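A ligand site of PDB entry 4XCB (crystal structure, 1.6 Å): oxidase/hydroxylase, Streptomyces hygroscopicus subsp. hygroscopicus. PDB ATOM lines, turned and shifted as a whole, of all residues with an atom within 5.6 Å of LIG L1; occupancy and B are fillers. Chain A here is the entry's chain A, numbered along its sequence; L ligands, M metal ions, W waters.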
ATOM      1  N   PHE A  49     -19.455  -6.539  10.845  1.00  0.00           N
ATOM      2  CA  PHE A  49     -18.438  -7.212  11.646  1.00  0.00           C
ATOM      3  C   PHE A  49     -18.867  -8.672  11.753  1.00  0.00           C
ATOM      4  O   PHE A  49     -20.028  -8.951  12.042  1.00  0.00           O
ATOM      5  CB  PHE A  49     -18.285  -6.584  13.031  1.00  0.00           C
ATOM      6  CG  PHE A  49     -18.063  -5.098  12.997  1.00  0.00           C
ATOM      7  CD2 PHE A  49     -16.781  -4.574  13.082  1.00  0.00           C
ATOM      8  CE2 PHE A  49     -16.589  -3.213  13.047  1.00  0.00           C
ATOM      9  N   ARG A  54     -26.524  -6.345  15.000  1.00  0.00           N
ATOM     10  CA  ARG A  54     -26.805  -5.068  15.645  1.00  0.00           C
ATOM     11  C   ARG A  54     -28.303  -4.749  15.647  1.00  0.00           C
ATOM     12  O   ARG A  54     -28.984  -4.899  14.632  1.00  0.00           O
ATOM     13  CB  ARG A  54     -26.022  -3.941  14.964  1.00  0.00           C
ATOM     14  CG  ARG A  54     -26.099  -2.585  15.651  1.00  0.00           C
ATOM     15  CD  ARG A  54     -25.110  -1.627  15.015  1.00  0.00           C
ATOM     16  NE  ARG A  54     -25.370  -0.235  15.375  1.00  0.00           N
ATOM     17  CZ  ARG A  54     -24.470   0.574  15.924  1.00  0.00           C
ATOM     18  NH1 ARG A  54     -23.254   0.133  16.176  1.00  0.00           N
ATOM     19  NH2 ARG A  54     -24.796   1.821  16.213  1.00  0.00           N
ATOM     20  N   GLU A  90     -28.112   8.170  20.630  1.00  0.00           N
ATOM     21  CA  GLU A  90     -28.274   6.865  20.004  1.00  0.00           C
ATOM     22  C   GLU A  90     -28.637   5.800  21.035  1.00  0.00           C
ATOM     23  O   GLU A  90     -28.403   5.970  22.218  1.00  0.00           O
ATOM     24  CB  GLU A  90     -27.004   6.431  19.267  1.00  0.00           C
ATOM     25  CG  GLU A  90     -25.768   6.462  20.143  1.00  0.00           C
ATOM     26  CD  GLU A  90     -24.538   5.964  19.424  1.00  0.00           C
ATOM     27  OE1 GLU A  90     -23.423   6.241  19.910  1.00  0.00           O
ATOM     28  OE2 GLU A  90     -24.667   5.276  18.382  1.00  0.00           O
ATOM     29  N   TYR A  92     -28.562   1.426  20.798  1.00  0.00           N
ATOM     30  CA  TYR A  92     -28.474   0.223  19.973  1.00  0.00           C
ATOM     31  C   TYR A  92     -28.142  -1.007  20.797  1.00  0.00           C
ATOM     32  O   TYR A  92     -27.797  -0.917  21.970  1.00  0.00           O
ATOM     33  CB  TYR A  92     -27.430   0.415  18.861  1.00  0.00           C
ATOM     34  CG  TYR A  92     -26.016   0.655  19.361  1.00  0.00           C
ATOM     35  CD1 TYR A  92     -25.570   1.943  19.621  1.00  0.00           C
ATOM     36  CD2 TYR A  92     -25.143  -0.399  19.537  1.00  0.00           C
ATOM     37  CE1 TYR A  92     -24.291   2.174  20.067  1.00  0.00           C
ATOM     38  CE2 TYR A  92     -23.862  -0.181  19.986  1.00  0.00           C
ATOM     39  CZ  TYR A  92     -23.440   1.111  20.242  1.00  0.00           C
ATOM     40  OH  TYR A  92     -22.154   1.328  20.682  1.00  0.00           O
ATOM     41  N   LEU A 102     -14.035  -6.716  18.480  1.00  0.00           N
ATOM     42  CA  LEU A 102     -14.229  -5.288  18.208  1.00  0.00           C
ATOM     43  C   LEU A 102     -12.912  -4.567  18.383  1.00  0.00           C
ATOM     44  O   LEU A 102     -12.406  -4.432  19.501  1.00  0.00           O
ATOM     45  CB  LEU A 102     -15.308  -4.697  19.124  1.00  0.00           C
ATOM     46  CG  LEU A 102     -15.810  -3.298  18.781  1.00  0.00           C
ATOM     47  CD1 LEU A 102     -16.380  -3.281  17.389  1.00  0.00           C
ATOM     48  CD2 LEU A 102     -16.872  -2.885  19.774  1.00  0.00           C
ATOM     49  N   TYR A 103     -12.347  -4.120  17.270  1.00  0.00           N
ATOM     50  CA  TYR A 103     -11.021  -3.511  17.298  1.00  0.00           C
ATOM     51  C   TYR A 103     -11.070  -2.143  17.964  1.00  0.00           C
ATOM     52  O   TYR A 103     -12.141  -1.539  18.066  1.00  0.00           O
ATOM     53  CB  TYR A 103     -10.476  -3.389  15.868  1.00  0.00           C
ATOM     54  CG  TYR A 103     -10.269  -4.714  15.168  1.00  0.00           C
ATOM     55  CD1 TYR A 103      -9.783  -5.812  15.867  1.00  0.00           C
ATOM     56  CD2 TYR A 103     -10.585  -4.874  13.830  1.00  0.00           C
ATOM     57  CE1 TYR A 103      -9.594  -7.023  15.234  1.00  0.00           C
ATOM     58  CE2 TYR A 103     -10.396  -6.084  13.197  1.00  0.00           C
ATOM     59  CZ  TYR A 103      -9.907  -7.150  13.906  1.00  0.00           C
ATOM     60  OH  TYR A 103      -9.710  -8.371  13.292  1.00  0.00           O
ATOM     61  N   LEU A 104      -9.909  -1.666  18.413  1.00  0.00           N
ATOM     62  CA  LEU A 104      -9.837  -0.409  19.156  1.00  0.00           C
ATOM     63  C   LEU A 104     -10.384   0.775  18.376  1.00  0.00           C
ATOM     64  O   LEU A 104     -10.226   0.892  17.147  1.00  0.00           O
ATOM     65  CB  LEU A 104      -8.391  -0.113  19.559  1.00  0.00           C
ATOM     66  CG  LEU A 104      -7.815  -1.109  20.560  1.00  0.00           C
ATOM     67  CD1 LEU A 104      -6.421  -0.642  21.036  1.00  0.00           C
ATOM     68  CD2 LEU A 104      -8.785  -1.339  21.730  1.00  0.00           C
ATOM     69  N   HIS A 105     -11.030   1.663  19.114  1.00  0.00           N
ATOM     70  CA  HIS A 105     -11.552   2.918  18.548  1.00  0.00           C
ATOM     71  C   HIS A 105     -11.571   3.953  19.642  1.00  0.00           C
ATOM     72  O   HIS A 105     -11.453   3.615  20.814  1.00  0.00           O
ATOM     73  CB  HIS A 105     -12.945   2.729  17.945  1.00  0.00           C
ATOM     74  CG  HIS A 105     -13.912   1.979  18.831  1.00  0.00           C
ATOM     75  ND1 HIS A 105     -13.933   0.607  18.911  1.00  0.00           N
ATOM     76  CD2 HIS A 105     -14.891   2.425  19.643  1.00  0.00           C
ATOM     77  CE1 HIS A 105     -14.885   0.236  19.760  1.00  0.00           C
ATOM     78  NE2 HIS A 105     -15.483   1.319  20.207  1.00  0.00           N
ATOM     79  N   TYR A 138     -19.547  13.376  25.022  1.00  0.00           N
ATOM     80  CA  TYR A 138     -20.135  12.185  24.429  1.00  0.00           C
ATOM     81  C   TYR A 138     -19.846  11.030  25.346  1.00  0.00           C
ATOM     82  O   TYR A 138     -18.689  10.605  25.458  1.00  0.00           O
ATOM     83  CB  TYR A 138     -19.570  11.922  23.025  1.00  0.00           C
ATOM     84  CG  TYR A 138     -20.471  11.102  22.124  1.00  0.00           C
ATOM     85  CD1 TYR A 138     -20.858  11.591  20.891  1.00  0.00           C
ATOM     86  CD2 TYR A 138     -20.942   9.859  22.511  1.00  0.00           C
ATOM     87  CE1 TYR A 138     -21.689  10.865  20.060  1.00  0.00           C
ATOM     88  CE2 TYR A 138     -21.766   9.113  21.688  1.00  0.00           C
ATOM     89  CZ  TYR A 138     -22.131   9.621  20.467  1.00  0.00           C
ATOM     90  OH  TYR A 138     -22.963   8.899  19.622  1.00  0.00           O
ATOM     91  N   LYS A 140     -21.395   7.074  26.889  1.00  0.00           N
ATOM     92  CA  LYS A 140     -22.263   5.943  26.682  1.00  0.00           C
ATOM     93  C   LYS A 140     -22.539   5.227  27.974  1.00  0.00           C
ATOM     94  O   LYS A 140     -21.651   5.097  28.820  1.00  0.00           O
ATOM     95  CB  LYS A 140     -21.648   4.962  25.694  1.00  0.00           C
ATOM     96  CG  LYS A 140     -21.784   5.344  24.271  1.00  0.00           C
ATOM     97  CD  LYS A 140     -21.382   4.187  23.396  1.00  0.00           C
ATOM     98  CE  LYS A 140     -21.326   4.611  21.952  1.00  0.00           C
ATOM     99  NZ  LYS A 140     -20.575   3.606  21.133  1.00  0.00           N
ATOM    100  N   GLU A 205     -16.327   8.571  25.668  1.00  0.00           N
ATOM    101  CA  GLU A 205     -16.006   8.054  24.333  1.00  0.00           C
ATOM    102  C   GLU A 205     -14.624   8.524  23.860  1.00  0.00           C
ATOM    103  O   GLU A 205     -14.121   8.062  22.835  1.00  0.00           O
ATOM    104  CB  GLU A 205     -17.099   8.430  23.332  1.00  0.00           C
ATOM    105  CG  GLU A 205     -18.301   7.478  23.419  1.00  0.00           C
ATOM    106  CD  GLU A 205     -17.960   6.056  22.984  1.00  0.00           C
ATOM    107  OE1 GLU A 205     -17.466   5.874  21.848  1.00  0.00           O
ATOM    108  OE2 GLU A 205     -18.174   5.120  23.779  1.00  0.00           O
ATOM    109  N   TRP A 235     -26.529  10.439  16.530  1.00  0.00           N
ATOM    110  CA  TRP A 235     -25.375   9.825  15.877  1.00  0.00           C
ATOM    111  C   TRP A 235     -25.683   9.316  14.465  1.00  0.00           C
ATOM    112  O   TRP A 235     -26.693   8.651  14.221  1.00  0.00           O
ATOM    113  CB  TRP A 235     -24.794   8.663  16.676  1.00  0.00           C
ATOM    114  CG  TRP A 235     -23.557   8.174  15.998  1.00  0.00           C
ATOM    115  CD1 TRP A 235     -22.312   8.736  16.075  1.00  0.00           C
ATOM    116  CD2 TRP A 235     -23.452   7.083  15.081  1.00  0.00           C
ATOM    117  NE1 TRP A 235     -21.429   8.040  15.286  1.00  0.00           N
ATOM    118  CE2 TRP A 235     -22.101   7.023  14.657  1.00  0.00           C
ATOM    119  CE3 TRP A 235     -24.352   6.139  14.579  1.00  0.00           C
ATOM    120  CZ2 TRP A 235     -21.646   6.055  13.765  1.00  0.00           C
ATOM    121  CZ3 TRP A 235     -23.891   5.180  13.689  1.00  0.00           C
ATOM    122  CH2 TRP A 235     -22.560   5.160  13.295  1.00  0.00           C
ATOM    123  N   GLU A 237     -23.011   8.104  10.948  1.00  0.00           N
ATOM    124  CA  GLU A 237     -21.675   8.019  10.384  1.00  0.00           C
ATOM    125  C   GLU A 237     -21.564   8.960   9.188  1.00  0.00           C
ATOM    126  O   GLU A 237     -22.452   9.012   8.355  1.00  0.00           O
ATOM    127  CB  GLU A 237     -21.368   6.580   9.953  1.00  0.00           C
ATOM    128  CG  GLU A 237     -19.986   6.413   9.360  1.00  0.00           C
ATOM    129  CD  GLU A 237     -19.633   4.955   9.159  1.00  0.00           C
ATOM    130  OE1 GLU A 237     -20.039   4.128  10.000  1.00  0.00           O
ATOM    131  OE2 GLU A 237     -18.961   4.635   8.154  1.00  0.00           O
ATOM    132  N   TYR A 250     -20.921  12.364  12.254  1.00  0.00           N
ATOM    133  CA  TYR A 250     -19.683  12.226  12.986  1.00  0.00           C
ATOM    134  C   TYR A 250     -18.619  11.616  12.087  1.00  0.00           C
ATOM    135  O   TYR A 250     -18.807  10.527  11.532  1.00  0.00           O
ATOM    136  CB  TYR A 250     -19.903  11.375  14.239  1.00  0.00           C
ATOM    137  CG  TYR A 250     -20.828  12.036  15.250  1.00  0.00           C
ATOM    138  CD1 TYR A 250     -22.187  12.167  14.998  1.00  0.00           C
ATOM    139  CD2 TYR A 250     -20.331  12.545  16.449  1.00  0.00           C
ATOM    140  CE1 TYR A 250     -23.037  12.784  15.908  1.00  0.00           C
ATOM    141  CE2 TYR A 250     -21.180  13.157  17.373  1.00  0.00           C
ATOM    142  CZ  TYR A 250     -22.531  13.254  17.095  1.00  0.00           C
ATOM    143  OH  TYR A 250     -23.382  13.875  17.991  1.00  0.00           O
ATOM    144  N   ASP A 252     -15.104  10.056  12.204  1.00  0.00           N
ATOM    145  CA  ASP A 252     -14.150   9.522  13.171  1.00  0.00           C
ATOM    146  C   ASP A 252     -12.703   9.699  12.727  1.00  0.00           C
ATOM    147  O   ASP A 252     -12.385   9.656  11.535  1.00  0.00           O
ATOM    148  CB  ASP A 252     -14.415   8.037  13.432  1.00  0.00           C
ATOM    149  CG  ASP A 252     -15.749   7.790  14.136  1.00  0.00           C
ATOM    150  OD1 ASP A 252     -16.406   8.752  14.586  1.00  0.00           O
ATOM    151  OD2 ASP A 252     -16.130   6.608  14.269  1.00  0.00           O
ATOM    152  N   HIS A 253     -11.839   9.874  13.717  1.00  0.00           N
ATOM    153  CA  HIS A 253     -10.398   9.868  13.505  1.00  0.00           C
ATOM    154  C   HIS A 253      -9.949   8.418  13.404  1.00  0.00           C
ATOM    155  O   HIS A 253     -10.793   7.527  13.421  1.00  0.00           O
ATOM    156  CB  HIS A 253      -9.693  10.641  14.634  1.00  0.00           C
ATOM    157  CG  HIS A 253      -9.995  12.101  14.625  1.00  0.00           C
ATOM    158  ND1 HIS A 253      -9.063  13.070  14.962  1.00  0.00           N
ATOM    159  CD2 HIS A 253     -11.122  12.783  14.310  1.00  0.00           C
ATOM    160  CE1 HIS A 253      -9.603  14.261  14.845  1.00  0.00           C
ATOM    161  NE2 HIS A 253     -10.858  14.118  14.463  1.00  0.00           N
ATOM    162  N   VAL A 255      -9.217   4.677  13.504  1.00  0.00           N
ATOM    163  CA  VAL A 255      -9.586   3.535  14.347  1.00  0.00           C
ATOM    164  C   VAL A 255      -8.889   2.302  13.772  1.00  0.00           C
ATOM    165  O   VAL A 255      -8.516   2.304  12.598  1.00  0.00           O
ATOM    166  CB  VAL A 255     -11.114   3.310  14.402  1.00  0.00           C
ATOM    167  CG1 VAL A 255     -11.809   4.531  15.018  1.00  0.00           C
ATOM    168  CG2 VAL A 255     -11.667   3.047  13.016  1.00  0.00           C
ATOM    169  N   GLU A 257      -9.979  -0.436  12.714  1.00  0.00           N
ATOM    170  CA  GLU A 257     -10.675  -0.917  11.521  1.00  0.00           C
ATOM    171  C   GLU A 257     -10.111  -0.321  10.225  1.00  0.00           C
ATOM    172  O   GLU A 257     -10.217  -0.946   9.165  1.00  0.00           O
ATOM    173  CB  GLU A 257     -12.179  -0.612  11.631  1.00  0.00           C
ATOM    174  CG  GLU A 257     -13.046  -1.342  10.630  1.00  0.00           C
ATOM    175  CD  GLU A 257     -14.513  -0.931  10.711  1.00  0.00           C
ATOM    176  OE1 GLU A 257     -14.923  -0.376  11.760  1.00  0.00           O
ATOM    177  OE2 GLU A 257     -15.251  -1.152   9.729  1.00  0.00           O
ATOM    178  N   ASP A 258      -9.508   0.868  10.303  1.00  0.00           N
ATOM    179  CA  ASP A 258      -8.914   1.508   9.131  1.00  0.00           C
ATOM    180  C   ASP A 258      -7.618   0.820   8.683  1.00  0.00           C
ATOM    181  O   ASP A 258      -7.205   0.984   7.535  1.00  0.00           O
ATOM    182  CB  ASP A 258      -8.575   2.979   9.412  1.00  0.00           C
ATOM    183  CG  ASP A 258      -9.787   3.845   9.681  1.00  0.00           C
ATOM    184  OD1 ASP A 258     -10.803   3.733   8.944  1.00  0.00           O
ATOM    185  OD2 ASP A 258      -9.712   4.654  10.630  1.00  0.00           O
HETATM  186  C1  LIG L   1     -15.720   4.363  11.764  1.00  0.00           C
HETATM  187  C2  LIG L   1     -14.926   4.263  10.478  1.00  0.00           C
HETATM  188  C3  LIG L   1     -15.805   3.718   9.366  1.00  0.00           C
HETATM  189  C4  LIG L   1     -16.365   2.350   9.748  1.00  0.00           C
HETATM  190  C5  LIG L   1     -17.083   2.398  11.094  1.00  0.00           C
HETATM  191  C6  LIG L   1     -16.245   3.013  12.180  1.00  0.00           C
HETATM  192  N1  LIG L   1     -14.456   5.553  10.144  1.00  0.00           N
HETATM  193  O1  LIG L   1     -14.850   4.834  12.772  1.00  0.00           O
HETATM  194  N2  LIG L   1     -17.275   1.941   8.740  1.00  0.00           N
HETATM  195  C7  LIG L   1     -16.514   1.392   7.612  1.00  0.00           C
HETATM  196  O2  LIG L   1     -17.374   1.067  11.471  1.00  0.00           O
HETATM  197  C8  LIG L   1     -17.251   3.210  15.760  1.00  0.00           C
HETATM  198  C9  LIG L   1     -16.504   2.729  14.551  1.00  0.00           C
HETATM  199  O3  LIG L   1     -16.384   1.335  14.474  1.00  0.00           O
HETATM  200  C10 LIG L   1     -15.727   0.825  15.601  1.00  0.00           C
HETATM  201  C11 LIG L   1     -16.692   0.893  16.738  1.00  0.00           C
HETATM  202  C12 LIG L   1     -17.026   2.426  16.977  1.00  0.00           C
HETATM  203  O4  LIG L   1     -17.096   3.184  13.342  1.00  0.00           O
HETATM  204  C13 LIG L   1     -15.320  -0.623  15.325  1.00  0.00           C
HETATM  205  O5  LIG L   1     -14.255  -0.621  14.367  1.00  0.00           O
HETATM  206  O6  LIG L   1     -17.849   0.216  16.433  1.00  0.00           O
HETATM  207  O7  LIG L   1     -18.133   2.499  17.761  1.00  0.00           O
HETATM  208  C14 LIG L   1     -19.073   3.339  17.060  1.00  0.00           C
HETATM  209  C15 LIG L   1     -20.456   2.863  17.339  1.00  0.00           C
HETATM  210  C16 LIG L   1     -21.466   3.911  16.887  1.00  0.00           C
HETATM  211  C17 LIG L   1     -21.158   5.266  17.482  1.00  0.00           C
HETATM  212  C18 LIG L   1     -19.778   5.642  17.083  1.00  0.00           C
HETATM  213  O8  LIG L   1     -18.892   4.646  17.552  1.00  0.00           O
HETATM  214  O9  LIG L   1     -18.728   3.278  15.608  1.00  0.00           O
HETATM  215  O10 LIG L   1     -20.747   1.669  16.608  1.00  0.00           O
HETATM  216  O11 LIG L   1     -22.762   3.458  17.234  1.00  0.00           O
HETATM  217  O12 LIG L   1     -21.266   5.255  18.912  1.00  0.00           O
HETATM  218  C19 LIG L   1     -19.368   6.981  17.726  1.00  0.00           C
HETATM  219  C20 LIG L   1     -18.229   7.593  16.942  1.00  0.00           C
HETATM  220  O13 LIG L   1     -18.679   8.144  15.718  1.00  0.00           O
HETATM  221  N3  LIG L   1     -18.905   6.739  19.032  1.00  0.00           N
HETATM  222  C1  LG2 L   2     -19.142   0.121  21.158  1.00  0.00           C
HETATM  223  O1  LG2 L   2     -18.678   1.193  20.658  1.00  0.00           O
HETATM  224  O2  LG2 L   2     -20.267  -0.337  20.780  1.00  0.00           O
HETATM  225  C2  LG2 L   2     -18.365  -0.614  22.207  1.00  0.00           C
HETATM  226  O3  LG2 L   2     -17.343  -0.077  22.624  1.00  0.00           O
HETATM  227  C3  LG2 L   2     -18.812  -1.981  22.679  1.00  0.00           C
HETATM  228  C4  LG2 L   2     -18.271  -2.372  24.037  1.00  0.00           C
HETATM  229  C5  LG2 L   2     -18.538  -3.843  24.294  1.00  0.00           C
HETATM  230  O4  LG2 L   2     -18.282  -4.334  25.438  1.00  0.00           O
HETATM  231  O5  LG2 L   2     -19.008  -4.556  23.377  1.00  0.00           O
HETATM  232 NI    NI M   1     -17.009   1.789  21.619  1.00  0.00          NI
HETATM  233  O   HOH W   1     -14.924   5.368  16.557  1.00  0.00           O
HETATM  234  O   HOH W   2     -13.347   8.627   9.368  1.00  0.00           O
HETATM  235  O   HOH W   3     -12.511   5.325   7.906  1.00  0.00           O
HETATM  236  O   HOH W   4     -19.954  -0.514  18.103  1.00  0.00           O
HETATM  237  O   HOH W   5     -17.437   3.598  20.858  1.00  0.00           O
HETATM  238  O   HOH W   6     -16.276   5.664  19.165  1.00  0.00           O
HETATM  239  O   HOH W   7     -11.652  -0.135  14.943  1.00  0.00           O
HETATM  240  O   HOH W   8     -18.490   9.277  20.077  1.00  0.00           O
HETATM  241  O   HOH W   9     -18.219  -0.917   8.972  1.00  0.00           O
HETATM  242  O   HOH W  10     -13.691  -3.699  14.479  1.00  0.00           O
HETATM  243  O   HOH W  11     -19.399   0.618  13.835  1.00  0.00           O
HETATM  244  O   HOH W  12     -11.976   6.152  11.254  1.00  0.00           O
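Water W7 lies within hydrogen-bond range of O5 of LIG L1, N of Glu 257, O of Leu 104 and O of Tyr 103. Water W4 bridges O2 of LG2 L2 and O10 of LIG L1. Water W6 lies within hydrogen-bond range of a nitrogen (N3) of LIG L1 and the side-chain carboxylate (OE1) of Glu 205. Water W9 lies within hydrogen-bond range of a nitrogen (N2) of LIG L1 (3.0 Å) and the side-chain carboxylate of Glu 257 (3.1 Å). Water W10 lies within hydrogen-bond range of the backbone NH (N) of Tyr 103 (3.1 Å) and an oxygen (O5) of LIG L1 (3.1 Å). Water W5 lies within hydrogen-bond range of the side-chain carboxylate of Glu 205 (2.5 Å), the side-chain amino group of Lys 140 (3.2 Å) and an oxygen (O7) of LIG L1 (3.4 Å).
The side-chain hydroxyl (OH) of Tyr 92 lies within hydrogen-bond range of an oxygen (O2) of LG2 L2. NZ of Lys 140 lies within salt-bridge range of O2 of LG2 L2 (3.97 Å). The indole nitrogen (NE1) of Trp 235 is in hydrogen-bond range of an oxygen (O13) of LIG L1. An oxygen (O13) of LIG L1 lies within hydrogen-bond range of the side-chain carboxylate (OD1) of Asp 252 (2.6 Å). An oxygen (O11) of LIG L1 is in hydrogen-bond range of the guanidinium group (NH2) of Arg 54 (2.8 Å). The side-chain carboxylate (OE2) of Glu 237 is in salt-bridge range of a nitrogen (N2) of LIG L1 (3.2 Å). A nitrogen (N3) of LIG L1 lies within salt-bridge range of the side-chain carboxylate (OE1) of Glu 205, 3.3 Å away. N2 of LIG L1 is in salt-bridge range of OE2 of Glu 257. OE1 of Glu 90 lies within hydrogen-bond range of O12 of LIG L1 (2.6 Å). The side-chain amino group (NZ) of Lys 140 lies within hydrogen-bond range of an oxygen (O12) of LIG L1.
A ring nitrogen (ND1) of His 105 is in hydrogen-bond range of the backbone carbonyl oxygen of Tyr 103. The backbone carbonyl oxygen (O) of Tyr 138 is in hydrogen-bond range of the backbone NH (N) of Glu 205, 3.1 Å away. NZ of Lys 140 lies within salt-bridge range of OE2 of Glu 205 (3.9 Å). NZ of Lys 140 lies within hydrogen-bond range of OH of Tyr 92 (2.8 Å). OE1 of Glu 90 lies within hydrogen-bond range of OH of Tyr 138, at 2.7 Å. The backbone NH (N) of Val 255 sits at hydrogen-bond distance from the side-chain carboxylate (OD2) of Asp 258 (2.9 Å).
Merely in contact with LIG L1: Phe 49, Tyr 92, Leu 102, His 105, Tyr 250 and Val 255. Hydrophobic or aromatic side chains that line LIG L1: Phe 49, Tyr 92, Leu 102, His 105, Trp 235, Tyr 250 and Val 255. Of the 19 residues printed, 14 come within 4 Å of LIG L1. Along chain A the residues within 4 Å of LIG L1 span positions 49 to 257.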
